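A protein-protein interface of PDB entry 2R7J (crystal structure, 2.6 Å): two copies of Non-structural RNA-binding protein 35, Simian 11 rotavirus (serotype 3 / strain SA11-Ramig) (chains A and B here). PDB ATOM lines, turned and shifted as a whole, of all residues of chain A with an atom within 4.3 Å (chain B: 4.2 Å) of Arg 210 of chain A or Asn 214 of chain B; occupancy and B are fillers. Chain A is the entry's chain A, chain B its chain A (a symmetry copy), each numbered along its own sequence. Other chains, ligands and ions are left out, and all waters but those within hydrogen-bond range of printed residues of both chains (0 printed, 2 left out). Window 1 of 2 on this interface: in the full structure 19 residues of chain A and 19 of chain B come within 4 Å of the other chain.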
ATOM      1  N   VAL A 206      -9.828   2.911  26.187  1.00  0.00           N
ATOM      2  CA  VAL A 206     -11.211   2.457  26.303  1.00  0.00           C
ATOM      3  C   VAL A 206     -12.186   3.559  25.870  1.00  0.00           C
ATOM      4  O   VAL A 206     -13.255   3.283  25.321  1.00  0.00           O
ATOM      5  CB  VAL A 206     -11.532   2.019  27.744  1.00  0.00           C
ATOM      6  CG1 VAL A 206     -13.029   1.773  27.904  1.00  0.00           C
ATOM      7  CG2 VAL A 206     -10.753   0.754  28.069  1.00  0.00           C
ATOM      8  N   ALA A 207     -11.815   4.809  26.098  1.00  0.00           N
ATOM      9  CA  ALA A 207     -12.695   5.888  25.697  1.00  0.00           C
ATOM     10  C   ALA A 207     -12.783   5.980  24.161  1.00  0.00           C
ATOM     11  O   ALA A 207     -13.861   6.184  23.601  1.00  0.00           O
ATOM     12  CB  ALA A 207     -12.210   7.206  26.294  1.00  0.00           C
ATOM     13  N   GLU A 208     -11.651   5.807  23.483  1.00  0.00           N
ATOM     14  CA  GLU A 208     -11.620   5.887  22.024  1.00  0.00           C
ATOM     15  C   GLU A 208     -12.400   4.735  21.368  1.00  0.00           C
ATOM     16  O   GLU A 208     -13.001   4.912  20.300  1.00  0.00           O
ATOM     17  CB  GLU A 208     -10.167   5.891  21.547  1.00  0.00           C
ATOM     18  CG  GLU A 208      -9.973   5.950  20.043  1.00  0.00           C
ATOM     19  CD  GLU A 208     -10.411   7.265  19.428  1.00  0.00           C
ATOM     20  OE1 GLU A 208     -10.551   8.283  20.159  1.00  0.00           O
ATOM     21  OE2 GLU A 208     -10.604   7.279  18.195  1.00  0.00           O
ATOM     22  N   LEU A 209     -12.392   3.567  22.010  1.00  0.00           N
ATOM     23  CA  LEU A 209     -13.102   2.401  21.487  1.00  0.00           C
ATOM     24  C   LEU A 209     -14.604   2.534  21.676  1.00  0.00           C
ATOM     25  O   LEU A 209     -15.385   2.137  20.805  1.00  0.00           O
ATOM     26  CB  LEU A 209     -12.605   1.119  22.164  1.00  0.00           C
ATOM     27  CG  LEU A 209     -11.188   0.717  21.733  1.00  0.00           C
ATOM     28  CD1 LEU A 209     -10.610  -0.306  22.689  1.00  0.00           C
ATOM     29  CD2 LEU A 209     -11.227   0.187  20.297  1.00  0.00           C
ATOM     30  N   ARG A 210     -15.014   3.096  22.809  1.00  0.00           N
ATOM     31  CA  ARG A 210     -16.434   3.273  23.076  1.00  0.00           C
ATOM     32  C   ARG A 210     -17.056   4.346  22.186  1.00  0.00           C
ATOM     33  O   ARG A 210     -18.163   4.177  21.675  1.00  0.00           O
ATOM     34  CB  ARG A 210     -16.654   3.620  24.547  1.00  0.00           C
ATOM     35  CG  ARG A 210     -16.489   2.428  25.469  1.00  0.00           C
ATOM     36  CD  ARG A 210     -16.630   2.812  26.932  1.00  0.00           C
ATOM     37  NE  ARG A 210     -16.458   1.654  27.810  1.00  0.00           N
ATOM     38  CZ  ARG A 210     -16.331   1.726  29.134  1.00  0.00           C
ATOM     39  NH1 ARG A 210     -16.357   2.906  29.749  1.00  0.00           N
ATOM     40  NH2 ARG A 210     -16.174   0.617  29.843  1.00  0.00           N
ATOM     41  N   TRP A 211     -16.328   5.438  21.981  1.00  0.00           N
ATOM     42  CA  TRP A 211     -16.814   6.554  21.178  1.00  0.00           C
ATOM     43  C   TRP A 211     -16.772   6.322  19.682  1.00  0.00           C
ATOM     44  O   TRP A 211     -17.799   6.375  18.997  1.00  0.00           O
ATOM     45  CB  TRP A 211     -16.010   7.818  21.494  1.00  0.00           C
ATOM     46  CG  TRP A 211     -16.353   8.961  20.603  1.00  0.00           C
ATOM     47  CD1 TRP A 211     -15.651   9.394  19.509  1.00  0.00           C
ATOM     48  CD2 TRP A 211     -17.531   9.777  20.675  1.00  0.00           C
ATOM     49  NE1 TRP A 211     -16.326  10.429  18.893  1.00  0.00           N
ATOM     50  CE2 TRP A 211     -17.483  10.681  19.587  1.00  0.00           C
ATOM     51  CE3 TRP A 211     -18.627   9.829  21.553  1.00  0.00           C
ATOM     52  CZ2 TRP A 211     -18.489  11.629  19.352  1.00  0.00           C
ATOM     53  CZ3 TRP A 211     -19.630  10.770  21.323  1.00  0.00           C
ATOM     54  CH2 TRP A 211     -19.553  11.657  20.229  1.00  0.00           C
ATOM     55  N   GLN A 212     -15.563   6.076  19.194  1.00  0.00           N
ATOM     56  CA  GLN A 212     -15.300   5.874  17.782  1.00  0.00           C
ATOM     57  C   GLN A 212     -15.659   4.504  17.238  1.00  0.00           C
ATOM     58  O   GLN A 212     -15.886   4.361  16.036  1.00  0.00           O
ATOM     59  CB  GLN A 212     -13.824   6.155  17.512  1.00  0.00           C
ATOM     60  CG  GLN A 212     -13.474   6.322  16.051  1.00  0.00           C
ATOM     61  CD  GLN A 212     -14.369   7.335  15.347  1.00  0.00           C
ATOM     62  OE1 GLN A 212     -14.586   8.452  15.839  1.00  0.00           O
ATOM     63  NE2 GLN A 212     -14.888   6.950  14.184  1.00  0.00           N
ATOM     64  N   ASN A 214     -18.180   2.094  18.815  1.00  0.00           N
ATOM     65  CA  ASN A 214     -19.213   1.465  19.640  1.00  0.00           C
ATOM     66  C   ASN A 214     -19.788   0.150  19.085  1.00  0.00           C
ATOM     67  O   ASN A 214     -20.165  -0.743  19.856  1.00  0.00           O
ATOM     68  CB  ASN A 214     -20.349   2.462  19.940  1.00  0.00           C
ATOM     69  CG  ASN A 214     -21.307   2.643  18.780  1.00  0.00           C
ATOM     70  OD1 ASN A 214     -20.922   3.087  17.701  1.00  0.00           O
ATOM     71  ND2 ASN A 214     -22.575   2.311  19.005  1.00  0.00           N
ATOM     72  N   PHE A 300     -14.187   1.810  34.327  1.00  0.00           N
ATOM     73  CA  PHE A 300     -14.318   3.241  34.054  1.00  0.00           C
ATOM     74  C   PHE A 300     -15.725   3.584  33.578  1.00  0.00           C
ATOM     75  O   PHE A 300     -16.432   2.747  32.992  1.00  0.00           O
ATOM     76  CB  PHE A 300     -13.311   3.708  32.990  1.00  0.00           C
ATOM     77  CG  PHE A 300     -12.019   2.941  32.977  1.00  0.00           C
ATOM     78  CD1 PHE A 300     -11.943   1.704  32.345  1.00  0.00           C
ATOM     79  CD2 PHE A 300     -10.868   3.479  33.544  1.00  0.00           C
ATOM     80  CE1 PHE A 300     -10.739   1.017  32.267  1.00  0.00           C
ATOM     81  CE2 PHE A 300      -9.652   2.797  33.470  1.00  0.00           C
ATOM     82  CZ  PHE A 300      -9.593   1.559  32.827  1.00  0.00           C
ATOM     83  N   LEU A 303     -16.967   8.158  30.515  1.00  0.00           N
ATOM     84  CA  LEU A 303     -16.087   8.415  29.379  1.00  0.00           C
ATOM     85  C   LEU A 303     -16.816   8.984  28.160  1.00  0.00           C
ATOM     86  O   LEU A 303     -16.403  10.009  27.605  1.00  0.00           O
ATOM     87  CB  LEU A 303     -15.352   7.135  28.980  1.00  0.00           C
ATOM     88  CG  LEU A 303     -14.366   6.604  30.017  1.00  0.00           C
ATOM     89  CD1 LEU A 303     -13.825   5.256  29.581  1.00  0.00           C
ATOM     90  CD2 LEU A 303     -13.241   7.607  30.213  1.00  0.00           C
ATOM     91  N   LEU B 209     -30.815   4.969  17.448  1.00  0.00           N
ATOM     92  CA  LEU B 209     -29.986   6.171  17.501  1.00  0.00           C
ATOM     93  C   LEU B 209     -28.750   5.957  18.358  1.00  0.00           C
ATOM     94  O   LEU B 209     -27.665   6.448  18.029  1.00  0.00           O
ATOM     95  CB  LEU B 209     -30.792   7.358  18.041  1.00  0.00           C
ATOM     96  CG  LEU B 209     -31.850   7.871  17.055  1.00  0.00           C
ATOM     97  CD1 LEU B 209     -32.849   8.764  17.761  1.00  0.00           C
ATOM     98  CD2 LEU B 209     -31.155   8.604  15.904  1.00  0.00           C
ATOM     99  N   ARG B 210     -28.905   5.219  19.453  1.00  0.00           N
ATOM    100  CA  ARG B 210     -27.775   4.952  20.332  1.00  0.00           C
ATOM    101  C   ARG B 210     -26.767   3.999  19.696  1.00  0.00           C
ATOM    102  O   ARG B 210     -25.556   4.200  19.802  1.00  0.00           O
ATOM    103  CB  ARG B 210     -28.266   4.385  21.663  1.00  0.00           C
ATOM    104  CG  ARG B 210     -28.893   5.435  22.560  1.00  0.00           C
ATOM    105  CD  ARG B 210     -29.447   4.835  23.840  1.00  0.00           C
ATOM    106  NE  ARG B 210     -30.058   5.858  24.691  1.00  0.00           N
ATOM    107  CZ  ARG B 210     -30.794   5.597  25.770  1.00  0.00           C
ATOM    108  NH1 ARG B 210     -31.019   4.339  26.143  1.00  0.00           N
ATOM    109  NH2 ARG B 210     -31.310   6.595  26.474  1.00  0.00           N
ATOM    110  N   GLN B 212     -26.598   2.784  16.137  1.00  0.00           N
ATOM    111  CA  GLN B 212     -26.168   3.200  14.816  1.00  0.00           C
ATOM    112  C   GLN B 212     -25.645   4.621  14.714  1.00  0.00           C
ATOM    113  O   GLN B 212     -24.881   4.931  13.799  1.00  0.00           O
ATOM    114  CB  GLN B 212     -27.329   3.017  13.841  1.00  0.00           C
ATOM    115  CG  GLN B 212     -26.938   3.079  12.382  1.00  0.00           C
ATOM    116  CD  GLN B 212     -25.779   2.148  12.046  1.00  0.00           C
ATOM    117  OE1 GLN B 212     -25.779   0.964  12.412  1.00  0.00           O
ATOM    118  NE2 GLN B 212     -24.786   2.679  11.338  1.00  0.00           N
ATOM    119  N   TYR B 213     -26.043   5.487  15.643  1.00  0.00           N
ATOM    120  CA  TYR B 213     -25.596   6.876  15.587  1.00  0.00           C
ATOM    121  C   TYR B 213     -25.091   7.435  16.914  1.00  0.00           C
ATOM    122  O   TYR B 213     -25.432   8.562  17.270  1.00  0.00           O
ATOM    123  CB  TYR B 213     -26.735   7.767  15.066  1.00  0.00           C
ATOM    124  CG  TYR B 213     -27.416   7.223  13.834  1.00  0.00           C
ATOM    125  CD1 TYR B 213     -28.505   6.353  13.936  1.00  0.00           C
ATOM    126  CD2 TYR B 213     -26.920   7.507  12.567  1.00  0.00           C
ATOM    127  CE1 TYR B 213     -29.076   5.772  12.796  1.00  0.00           C
ATOM    128  CE2 TYR B 213     -27.475   6.942  11.429  1.00  0.00           C
ATOM    129  CZ  TYR B 213     -28.549   6.075  11.543  1.00  0.00           C
ATOM    130  OH  TYR B 213     -29.085   5.522  10.403  1.00  0.00           O
ATOM    131  N   ASN B 214     -24.264   6.678  17.632  1.00  0.00           N
ATOM    132  CA  ASN B 214     -23.770   7.140  18.930  1.00  0.00           C
ATOM    133  C   ASN B 214     -23.049   8.500  18.913  1.00  0.00           C
ATOM    134  O   ASN B 214     -23.117   9.256  19.893  1.00  0.00           O
ATOM    135  CB  ASN B 214     -22.875   6.068  19.583  1.00  0.00           C
ATOM    136  CG  ASN B 214     -21.476   6.025  19.002  1.00  0.00           C
ATOM    137  OD1 ASN B 214     -21.287   5.757  17.818  1.00  0.00           O
ATOM    138  ND2 ASN B 214     -20.479   6.272  19.847  1.00  0.00           N
ATOM    139  N   LYS B 215     -22.388   8.826  17.803  1.00  0.00           N
ATOM    140  CA  LYS B 215     -21.682  10.099  17.683  1.00  0.00           C
ATOM    141  C   LYS B 215     -22.569  11.254  17.187  1.00  0.00           C
ATOM    142  O   LYS B 215     -22.065  12.251  16.650  1.00  0.00           O
ATOM    143  CB  LYS B 215     -20.474   9.919  16.753  1.00  0.00           C
ATOM    144  CG  LYS B 215     -19.407   8.985  17.345  1.00  0.00           C
ATOM    145  CD  LYS B 215     -18.246   8.693  16.399  1.00  0.00           C
ATOM    146  CE  LYS B 215     -18.637   7.713  15.316  1.00  0.00           C
ATOM    147  NZ  LYS B 215     -19.609   8.310  14.364  1.00  0.00           N
ATOM    148  N   PHE B 216     -23.884  11.124  17.362  1.00  0.00           N
ATOM    149  CA  PHE B 216     -24.828  12.156  16.916  1.00  0.00           C
ATOM    150  C   PHE B 216     -25.739  12.644  18.035  1.00  0.00           C
ATOM    151  O   PHE B 216     -26.183  11.858  18.873  1.00  0.00           O
ATOM    152  CB  PHE B 216     -25.717  11.648  15.762  1.00  0.00           C
ATOM    153  CG  PHE B 216     -25.014  11.560  14.433  1.00  0.00           C
ATOM    154  CD1 PHE B 216     -24.115  10.526  14.166  1.00  0.00           C
ATOM    155  CD2 PHE B 216     -25.223  12.539  13.455  1.00  0.00           C
ATOM    156  CE1 PHE B 216     -23.430  10.472  12.944  1.00  0.00           C
ATOM    157  CE2 PHE B 216     -24.546  12.496  12.233  1.00  0.00           C
ATOM    158  CZ  PHE B 216     -23.643  11.461  11.975  1.00  0.00           C
ATOM    159  N   TYR B 231     -22.290  15.924  17.205  1.00  0.00           N
ATOM    160  CA  TYR B 231     -22.126  16.692  18.436  1.00  0.00           C
ATOM    161  C   TYR B 231     -21.263  17.926  18.207  1.00  0.00           C
ATOM    162  O   TYR B 231     -21.437  18.938  18.869  1.00  0.00           O
ATOM    163  CB  TYR B 231     -21.503  15.821  19.527  1.00  0.00           C
ATOM    164  CG  TYR B 231     -22.524  14.978  20.260  1.00  0.00           C
ATOM    165  CD1 TYR B 231     -23.349  15.539  21.236  1.00  0.00           C
ATOM    166  CD2 TYR B 231     -22.687  13.629  19.962  1.00  0.00           C
ATOM    167  CE1 TYR B 231     -24.311  14.769  21.892  1.00  0.00           C
ATOM    168  CE2 TYR B 231     -23.642  12.856  20.616  1.00  0.00           C
ATOM    169  CZ  TYR B 231     -24.444  13.431  21.574  1.00  0.00           C
ATOM    170  OH  TYR B 231     -25.369  12.663  22.224  1.00  0.00           O
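Of the printed residues of chain B, Arg 210 of chain A touches Asn 214.
Of the printed residues of chain B, Gln 212 of chain A touches Lys 215 (3.7 Å).
Of the printed residues of chain B, Asn 214 of chain A touches Arg 210 and Asn 214.
Asn 214 of chain B touches just these residues of chain A: Arg 210 (3.6 Å), Trp 211 (2.8 Å) and Asn 214 (2.7 Å).
Of the printed residues of chain A, Lys 215 of chain B touches Trp 211 (3.4 Å) and Gln 212 (3.7 Å).
Phe 216 of chain B touches none of the printed residues of chain A.
The nearest printed residue of chain B that does not touch Arg 210 of chain A is Lys 215 of chain B (6.6 Å).
The nearest printed residue of chain A that does not touch Tyr 231 of chain B is Arg 210 of chain A (10.3 Å).
Hydrophobic or aromatic side chains of chain A within 4 Å of the printed part of chain B: Trp 211.
Along chain A the printed residues that touch a printed residue of chain B span positions 210 to 214.
Hydrophobic or aromatic side chains of chain B that line the printed part of chain A: Tyr 231.
Along chain B the printed residues that touch a printed residue of chain A span positions 210 to 231.
Among the printed residues, no Asp or Glu carboxylate lies within 4 Å of a Lys or Arg side-chain nitrogen of the other chain.
O of Leu 209 of chain A sits at hydrogen-bond distance from N of Asn 214 of chain A (3.4 Å).
O of Leu 209 of chain B is in hydrogen-bond range of N of Asn 214 of chain B (3.4 Å).
NH1 of Arg 210 of chain A lies within hydrogen-bond range of O of Phe 300 of chain A (3.2 Å).
The backbone carbonyl oxygen (O) of Trp 211 of chain A lies within hydrogen-bond range of the side-chain amide nitrogen (ND2) of Asn 214 of chain B (2.8 Å).
The side-chain amide oxygen of Asn 214 of chain A sits close to the side-chain amide oxygen of Asn 214 of chain B.
Among the printed residues, pairs that only touch across the chains: Trp 211 of chain A with Lys 215 of chain B, Asn 214 of chain A with Arg 210 of chain B, Arg 210 of chain A with Asn 214 of chain B, Gln 212 of chain A with Lys 215 of chain B and Trp 211 of chain A with Tyr 231 of chain B.
Arg 210 of chain A touches Asn 214 of chain B, and with the chains exchanged Asn 214 of chain A touches Arg 210 of chain B.
Asn 214 of chain A touches its own counterpart, Asn 214 of chain B.
Positions printed for both chains: 209, 210, 212 and 214.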
